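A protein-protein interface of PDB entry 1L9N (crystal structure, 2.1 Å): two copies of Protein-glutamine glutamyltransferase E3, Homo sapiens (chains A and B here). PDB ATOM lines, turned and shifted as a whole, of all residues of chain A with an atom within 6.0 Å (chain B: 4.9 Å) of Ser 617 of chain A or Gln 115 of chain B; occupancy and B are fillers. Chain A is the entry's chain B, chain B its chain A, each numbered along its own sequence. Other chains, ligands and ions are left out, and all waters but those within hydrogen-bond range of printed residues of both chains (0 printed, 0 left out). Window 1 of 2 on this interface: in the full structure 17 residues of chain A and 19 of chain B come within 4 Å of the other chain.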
ATOM      1  N   PRO A 594      28.995  -2.712   9.530  1.00  0.00           N
ATOM      2  CA  PRO A 594      28.946  -2.435  10.969  1.00  0.00           C
ATOM      3  C   PRO A 594      30.330  -2.781  11.519  1.00  0.00           C
ATOM      4  O   PRO A 594      31.090  -3.513  10.880  1.00  0.00           O
ATOM      5  CB  PRO A 594      27.850  -3.378  11.474  1.00  0.00           C
ATOM      6  CG  PRO A 594      27.835  -4.484  10.465  1.00  0.00           C
ATOM      7  CD  PRO A 594      28.024  -3.751   9.154  1.00  0.00           C
ATOM      8  N   THR A 595      30.672  -2.271  12.689  1.00  0.00           N
ATOM      9  CA  THR A 595      31.995  -2.539  13.226  1.00  0.00           C
ATOM     10  C   THR A 595      32.257  -3.985  13.632  1.00  0.00           C
ATOM     11  O   THR A 595      31.346  -4.720  14.001  1.00  0.00           O
ATOM     12  CB  THR A 595      32.290  -1.647  14.434  1.00  0.00           C
ATOM     13  OG1 THR A 595      32.027  -0.282  14.090  1.00  0.00           O
ATOM     14  CG2 THR A 595      33.756  -1.775  14.839  1.00  0.00           C
ATOM     15  N   LEU A 615      34.433  -8.912  18.766  1.00  0.00           N
ATOM     16  CA  LEU A 615      33.236  -8.178  19.148  1.00  0.00           C
ATOM     17  C   LEU A 615      32.464  -7.706  17.922  1.00  0.00           C
ATOM     18  O   LEU A 615      32.990  -6.966  17.088  1.00  0.00           O
ATOM     19  CB  LEU A 615      33.618  -6.964  19.995  1.00  0.00           C
ATOM     20  CG  LEU A 615      34.479  -7.227  21.234  1.00  0.00           C
ATOM     21  CD1 LEU A 615      34.933  -5.897  21.827  1.00  0.00           C
ATOM     22  CD2 LEU A 615      33.693  -8.044  22.252  1.00  0.00           C
ATOM     23  N   PHE A 616      31.218  -8.147  17.807  1.00  0.00           N
ATOM     24  CA  PHE A 616      30.363  -7.735  16.703  1.00  0.00           C
ATOM     25  C   PHE A 616      28.931  -7.568  17.189  1.00  0.00           C
ATOM     26  O   PHE A 616      28.420  -8.409  17.928  1.00  0.00           O
ATOM     27  CB  PHE A 616      30.363  -8.765  15.576  1.00  0.00           C
ATOM     28  CG  PHE A 616      29.373  -8.452  14.485  1.00  0.00           C
ATOM     29  CD1 PHE A 616      29.676  -7.522  13.498  1.00  0.00           C
ATOM     30  CD2 PHE A 616      28.113  -9.042  14.482  1.00  0.00           C
ATOM     31  CE1 PHE A 616      28.739  -7.186  12.526  1.00  0.00           C
ATOM     32  CE2 PHE A 616      27.171  -8.712  13.517  1.00  0.00           C
ATOM     33  CZ  PHE A 616      27.484  -7.782  12.535  1.00  0.00           C
ATOM     34  N   SER A 617      28.286  -6.484  16.771  1.00  0.00           N
ATOM     35  CA  SER A 617      26.901  -6.234  17.150  1.00  0.00           C
ATOM     36  C   SER A 617      26.017  -6.114  15.915  1.00  0.00           C
ATOM     37  O   SER A 617      26.355  -5.414  14.959  1.00  0.00           O
ATOM     38  CB  SER A 617      26.794  -4.961  17.996  1.00  0.00           C
ATOM     39  OG  SER A 617      27.081  -5.236  19.356  1.00  0.00           O
ATOM     40  N   ASN A 618      24.887  -6.809  15.935  1.00  0.00           N
ATOM     41  CA  ASN A 618      23.945  -6.784  14.819  1.00  0.00           C
ATOM     42  C   ASN A 618      23.050  -5.547  14.885  1.00  0.00           C
ATOM     43  O   ASN A 618      22.223  -5.414  15.784  1.00  0.00           O
ATOM     44  CB  ASN A 618      23.099  -8.054  14.840  1.00  0.00           C
ATOM     45  CG  ASN A 618      22.125  -8.126  13.683  1.00  0.00           C
ATOM     46  OD1 ASN A 618      22.249  -7.386  12.707  1.00  0.00           O
ATOM     47  ND2 ASN A 618      21.157  -9.032  13.782  1.00  0.00           N
ATOM     48  N   PRO A 619      23.207  -4.617  13.933  1.00  0.00           N
ATOM     49  CA  PRO A 619      22.379  -3.407  13.947  1.00  0.00           C
ATOM     50  C   PRO A 619      21.001  -3.566  13.301  1.00  0.00           C
ATOM     51  O   PRO A 619      20.153  -2.684  13.434  1.00  0.00           O
ATOM     52  CB  PRO A 619      23.239  -2.403  13.192  1.00  0.00           C
ATOM     53  CG  PRO A 619      23.849  -3.274  12.119  1.00  0.00           C
ATOM     54  CD  PRO A 619      24.250  -4.530  12.892  1.00  0.00           C
ATOM     55  N   LEU A 648      22.681 -14.777  15.335  1.00  0.00           N
ATOM     56  CA  LEU A 648      22.690 -13.625  16.220  1.00  0.00           C
ATOM     57  C   LEU A 648      21.438 -12.773  16.019  1.00  0.00           C
ATOM     58  O   LEU A 648      21.254 -12.156  14.966  1.00  0.00           O
ATOM     59  CB  LEU A 648      23.948 -12.799  15.948  1.00  0.00           C
ATOM     60  CG  LEU A 648      24.297 -11.643  16.883  1.00  0.00           C
ATOM     61  CD1 LEU A 648      24.489 -12.176  18.304  1.00  0.00           C
ATOM     62  CD2 LEU A 648      25.572 -10.956  16.388  1.00  0.00           C
ATOM     63  N   LYS A 651      19.910  -6.551  17.077  1.00  0.00           N
ATOM     64  CA  LYS A 651      20.472  -5.672  18.097  1.00  0.00           C
ATOM     65  C   LYS A 651      21.364  -6.403  19.102  1.00  0.00           C
ATOM     66  O   LYS A 651      21.805  -5.812  20.086  1.00  0.00           O
ATOM     67  CB  LYS A 651      19.348  -4.957  18.853  1.00  0.00           C
ATOM     68  CG  LYS A 651      18.343  -4.216  17.978  1.00  0.00           C
ATOM     69  CD  LYS A 651      19.010  -3.148  17.126  1.00  0.00           C
ATOM     70  CE  LYS A 651      17.984  -2.266  16.438  1.00  0.00           C
ATOM     71  NZ  LYS A 651      17.046  -3.065  15.610  1.00  0.00           N
ATOM     72  N   GLU A 652      21.649  -7.676  18.856  1.00  0.00           N
ATOM     73  CA  GLU A 652      22.464  -8.447  19.787  1.00  0.00           C
ATOM     74  C   GLU A 652      23.958  -8.479  19.462  1.00  0.00           C
ATOM     75  O   GLU A 652      24.364  -8.258  18.323  1.00  0.00           O
ATOM     76  CB  GLU A 652      21.908  -9.864  19.888  1.00  0.00           C
ATOM     77  CG  GLU A 652      20.424  -9.877  20.227  1.00  0.00           C
ATOM     78  CD  GLU A 652      19.901 -11.259  20.549  1.00  0.00           C
ATOM     79  OE1 GLU A 652      18.665 -11.416  20.659  1.00  0.00           O
ATOM     80  OE2 GLU A 652      20.725 -12.187  20.699  1.00  0.00           O
ATOM     81  N   ARG A 653      24.774  -8.751  20.476  1.00  0.00           N
ATOM     82  CA  ARG A 653      26.217  -8.795  20.292  1.00  0.00           C
ATOM     83  C   ARG A 653      26.754 -10.207  20.333  1.00  0.00           C
ATOM     84  O   ARG A 653      26.337 -11.025  21.150  1.00  0.00           O
ATOM     85  CB  ARG A 653      26.937  -7.974  21.361  1.00  0.00           C
ATOM     86  CG  ARG A 653      26.837  -8.557  22.762  1.00  0.00           C
ATOM     87  CD  ARG A 653      25.626  -8.008  23.513  1.00  0.00           C
ATOM     88  NE  ARG A 653      25.405  -8.671  24.798  1.00  0.00           N
ATOM     89  CZ  ARG A 653      26.359  -8.909  25.693  1.00  0.00           C
ATOM     90  NH1 ARG A 653      27.611  -8.540  25.443  1.00  0.00           N
ATOM     91  NH2 ARG A 653      26.058  -9.514  26.838  1.00  0.00           N
ATOM     92  N   SER A 654      27.692 -10.484  19.441  1.00  0.00           N
ATOM     93  CA  SER A 654      28.310 -11.793  19.383  1.00  0.00           C
ATOM     94  C   SER A 654      29.640 -11.705  20.111  1.00  0.00           C
ATOM     95  O   SER A 654      30.477 -10.862  19.793  1.00  0.00           O
ATOM     96  CB  SER A 654      28.529 -12.210  17.929  1.00  0.00           C
ATOM     97  OG  SER A 654      29.250 -13.425  17.849  1.00  0.00           O
ATOM     98  N   ARG B  52      17.525   0.928  21.128  1.00  0.00           N
ATOM     99  CA  ARG B  52      18.002   0.202  22.298  1.00  0.00           C
ATOM    100  C   ARG B  52      19.313   0.739  22.857  1.00  0.00           C
ATOM    101  O   ARG B  52      20.239   1.057  22.109  1.00  0.00           O
ATOM    102  CB  ARG B  52      18.153  -1.275  21.938  1.00  0.00           C
ATOM    103  CG  ARG B  52      18.783  -2.145  23.007  1.00  0.00           C
ATOM    104  CD  ARG B  52      18.840  -3.578  22.508  1.00  0.00           C
ATOM    105  NE  ARG B  52      19.507  -4.482  23.433  1.00  0.00           N
ATOM    106  CZ  ARG B  52      19.577  -5.799  23.254  1.00  0.00           C
ATOM    107  NH1 ARG B  52      19.015  -6.354  22.186  1.00  0.00           N
ATOM    108  NH2 ARG B  52      20.210  -6.562  24.141  1.00  0.00           N
ATOM    109  N   LEU B  53      19.381   0.833  24.181  1.00  0.00           N
ATOM    110  CA  LEU B  53      20.574   1.325  24.855  1.00  0.00           C
ATOM    111  C   LEU B  53      21.232   0.201  25.633  1.00  0.00           C
ATOM    112  O   LEU B  53      20.572  -0.490  26.414  1.00  0.00           O
ATOM    113  CB  LEU B  53      20.217   2.447  25.827  1.00  0.00           C
ATOM    114  CG  LEU B  53      19.494   3.671  25.271  1.00  0.00           C
ATOM    115  CD1 LEU B  53      19.192   4.631  26.405  1.00  0.00           C
ATOM    116  CD2 LEU B  53      20.350   4.337  24.214  1.00  0.00           C
ATOM    117  N   GLU B  54      22.530   0.022  25.413  1.00  0.00           N
ATOM    118  CA  GLU B  54      23.295  -1.004  26.104  1.00  0.00           C
ATOM    119  C   GLU B  54      24.432  -0.335  26.862  1.00  0.00           C
ATOM    120  O   GLU B  54      25.279   0.333  26.265  1.00  0.00           O
ATOM    121  CB  GLU B  54      23.863  -2.016  25.104  1.00  0.00           C
ATOM    122  CG  GLU B  54      22.801  -2.836  24.392  1.00  0.00           C
ATOM    123  CD  GLU B  54      22.781  -4.292  24.817  1.00  0.00           C
ATOM    124  OE1 GLU B  54      22.921  -4.569  26.029  1.00  0.00           O
ATOM    125  OE2 GLU B  54      22.609  -5.165  23.938  1.00  0.00           O
ATOM    126  N   ILE B  56      27.879  -0.240  28.969  1.00  0.00           N
ATOM    127  CA  ILE B  56      29.120  -1.000  29.001  1.00  0.00           C
ATOM    128  C   ILE B  56      30.072  -0.468  30.064  1.00  0.00           C
ATOM    129  O   ILE B  56      30.491   0.693  30.011  1.00  0.00           O
ATOM    130  CB  ILE B  56      29.848  -0.944  27.645  1.00  0.00           C
ATOM    131  CG1 ILE B  56      28.923  -1.445  26.539  1.00  0.00           C
ATOM    132  CG2 ILE B  56      31.110  -1.795  27.696  1.00  0.00           C
ATOM    133  CD1 ILE B  56      29.515  -1.332  25.149  1.00  0.00           C
ATOM    134  N   ALA B 113      30.475   3.251  29.157  1.00  0.00           N
ATOM    135  CA  ALA B 113      30.175   3.678  27.801  1.00  0.00           C
ATOM    136  C   ALA B 113      28.741   3.300  27.461  1.00  0.00           C
ATOM    137  O   ALA B 113      28.145   2.432  28.112  1.00  0.00           O
ATOM    138  CB  ALA B 113      31.137   3.022  26.818  1.00  0.00           C
ATOM    139  N   LEU B 114      28.184   3.960  26.451  1.00  0.00           N
ATOM    140  CA  LEU B 114      26.817   3.676  26.035  1.00  0.00           C
ATOM    141  C   LEU B 114      26.749   3.280  24.572  1.00  0.00           C
ATOM    142  O   LEU B 114      27.221   4.010  23.697  1.00  0.00           O
ATOM    143  CB  LEU B 114      25.923   4.889  26.263  1.00  0.00           C
ATOM    144  CG  LEU B 114      24.433   4.638  26.021  1.00  0.00           C
ATOM    145  CD1 LEU B 114      23.917   3.619  27.028  1.00  0.00           C
ATOM    146  CD2 LEU B 114      23.668   5.940  26.150  1.00  0.00           C
ATOM    147  N   GLN B 115      26.182   2.109  24.308  1.00  0.00           N
ATOM    148  CA  GLN B 115      26.035   1.643  22.937  1.00  0.00           C
ATOM    149  C   GLN B 115      24.590   1.945  22.563  1.00  0.00           C
ATOM    150  O   GLN B 115      23.668   1.609  23.310  1.00  0.00           O
ATOM    151  CB  GLN B 115      26.312   0.142  22.829  1.00  0.00           C
ATOM    152  CG  GLN B 115      26.743  -0.278  21.430  1.00  0.00           C
ATOM    153  CD  GLN B 115      26.953  -1.781  21.276  1.00  0.00           C
ATOM    154  OE1 GLN B 115      27.740  -2.217  20.438  1.00  0.00           O
ATOM    155  NE2 GLN B 115      26.238  -2.576  22.067  1.00  0.00           N
ATOM    156  N   ILE B 116      24.400   2.589  21.417  1.00  0.00           N
ATOM    157  CA  ILE B 116      23.067   2.962  20.965  1.00  0.00           C
ATOM    158  C   ILE B 116      22.680   2.363  19.623  1.00  0.00           C
ATOM    159  O   ILE B 116      23.386   2.529  18.622  1.00  0.00           O
ATOM    160  CB  ILE B 116      22.930   4.494  20.827  1.00  0.00           C
ATOM    161  CG1 ILE B 116      23.226   5.174  22.158  1.00  0.00           C
ATOM    162  CG2 ILE B 116      21.523   4.849  20.359  1.00  0.00           C
ATOM    163  CD1 ILE B 116      23.200   6.685  22.077  1.00  0.00           C
ATOM    164  N   PHE B 117      21.544   1.681  19.615  1.00  0.00           N
ATOM    165  CA  PHE B 117      21.005   1.073  18.412  1.00  0.00           C
ATOM    166  C   PHE B 117      19.854   1.962  17.951  1.00  0.00           C
ATOM    167  O   PHE B 117      18.811   2.025  18.604  1.00  0.00           O
ATOM    168  CB  PHE B 117      20.487  -0.332  18.719  1.00  0.00           C
ATOM    169  CG  PHE B 117      21.573  -1.314  19.053  1.00  0.00           C
ATOM    170  CD1 PHE B 117      21.959  -2.282  18.131  1.00  0.00           C
ATOM    171  CD2 PHE B 117      22.223  -1.261  20.283  1.00  0.00           C
ATOM    172  CE1 PHE B 117      22.979  -3.189  18.427  1.00  0.00           C
ATOM    173  CE2 PHE B 117      23.249  -2.165  20.588  1.00  0.00           C
ATOM    174  CZ  PHE B 117      23.625  -3.131  19.655  1.00  0.00           C
ATOM    175  N   ILE B 122      24.441   1.776  14.596  1.00  0.00           N
ATOM    176  CA  ILE B 122      24.900   1.635  15.966  1.00  0.00           C
ATOM    177  C   ILE B 122      25.922   2.716  16.258  1.00  0.00           C
ATOM    178  O   ILE B 122      26.743   3.050  15.402  1.00  0.00           O
ATOM    179  CB  ILE B 122      25.581   0.271  16.208  1.00  0.00           C
ATOM    180  CG1 ILE B 122      24.630  -0.868  15.839  1.00  0.00           C
ATOM    181  CG2 ILE B 122      25.997   0.152  17.674  1.00  0.00           C
ATOM    182  CD1 ILE B 122      25.247  -2.245  16.011  1.00  0.00           C
ATOM    183  N   SER B 123      25.860   3.272  17.461  1.00  0.00           N
ATOM    184  CA  SER B 123      26.807   4.300  17.870  1.00  0.00           C
ATOM    185  C   SER B 123      27.299   3.972  19.271  1.00  0.00           C
ATOM    186  O   SER B 123      26.615   3.282  20.033  1.00  0.00           O
ATOM    187  CB  SER B 123      26.154   5.683  17.866  1.00  0.00           C
ATOM    188  OG  SER B 123      25.124   5.772  18.835  1.00  0.00           O
ATOM    189  N   SER B 124      28.487   4.461  19.605  1.00  0.00           N
ATOM    190  CA  SER B 124      29.053   4.218  20.920  1.00  0.00           C
ATOM    191  C   SER B 124      29.753   5.468  21.441  1.00  0.00           C
ATOM    192  O   SER B 124      30.508   6.120  20.712  1.00  0.00           O
ATOM    193  CB  SER B 124      30.045   3.055  20.859  1.00  0.00           C
ATOM    194  OG  SER B 124      30.642   2.832  22.123  1.00  0.00           O
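Along chain A the printed residues that touch a printed residue of chain B span positions 617 to 651. Of the 12 printed residues of chain B, 5 touch a printed residue of chain A. Printed residues of chain B that touch a printed residue of chain A: Arg 52, Glu 54, Gln 115, Phe 117 and Ile 122. Hydrophobic or aromatic side chains of chain B that line the printed part of chain A: Phe 117 and Ile 122. Among the printed residues, no Asp or Glu carboxylate lies within 4 Å of a Lys or Arg side-chain nitrogen of the other chain.
The backbone carbonyl oxygen of Asn 618 of chain A lies within hydrogen-bond range of the backbone NH of Lys 651 of chain A (2.9 Å). O of Leu 648 of chain A is in hydrogen-bond range of ND2 of Asn 618 of chain A (3.3 Å). The side-chain carboxylate (OE2) of Glu 54 of chain B lies within salt-bridge range of the guanidinium group (NH2) of Arg 52 of chain B (2.8 Å). The backbone carbonyl oxygen (O) of Arg 52 of chain B is in hydrogen-bond range of the backbone NH (N) of Phe 117 of chain B (2.9 Å). The backbone NH (N) of Asn 618 of chain A lies within hydrogen-bond range of the backbone carbonyl oxygen (O) of Glu 652 of chain A (2.8 Å). O of Glu 54 of chain B is in hydrogen-bond range of N of Gln 115 of chain B, at 2.8 Å.
Of the printed residues of chain B, Ser 617 of chain A touches Gln 115 (3.3 Å) and Ile 122 (3.5 Å). Of the printed residues of chain B, Pro 619 of chain A touches Ile 122 (3.4 Å). Of the printed residues of chain A, Glu 54 of chain B touches Lys 651 (3.99 Å). Printed residues of chain A within 4 Å of Gln 115 of chain B: Ser 617. Printed residues of chain A within 4 Å of Phe 117 of chain B: Asn 618 (3.5 Å) and Lys 651 (3.2 Å). Of the printed residues of chain A, Ile 122 of chain B touches Ser 617 and Pro 619. The nearest residue of chain A that does not touch Gln 115 of chain B is Arg 653 of chain A (5.5 Å). The nearest printed residue of chain A that does not touch Phe 117 of chain B is Ser 617 of chain A (4.02 Å).
Ser 617 of chain A touches Ile 122 of chain B (O to CD1, 3.5 Å). Asn 618 of chain A touches Phe 117 of chain B (O to CE1, 3.5 Å). Pro 619 of chain A touches Ile 122 of chain B. Arg 52 of chain B touches Lys 651 of chain A. Lys 651 of chain A touches Glu 54 of chain B. Phe 117 of chain B touches Lys 651 of chain A.
No position is printed for both chains.
OG of Ser 617 of chain A lies within hydrogen-bond range of OE1 of Gln 115 of chain B (3.3 Å).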
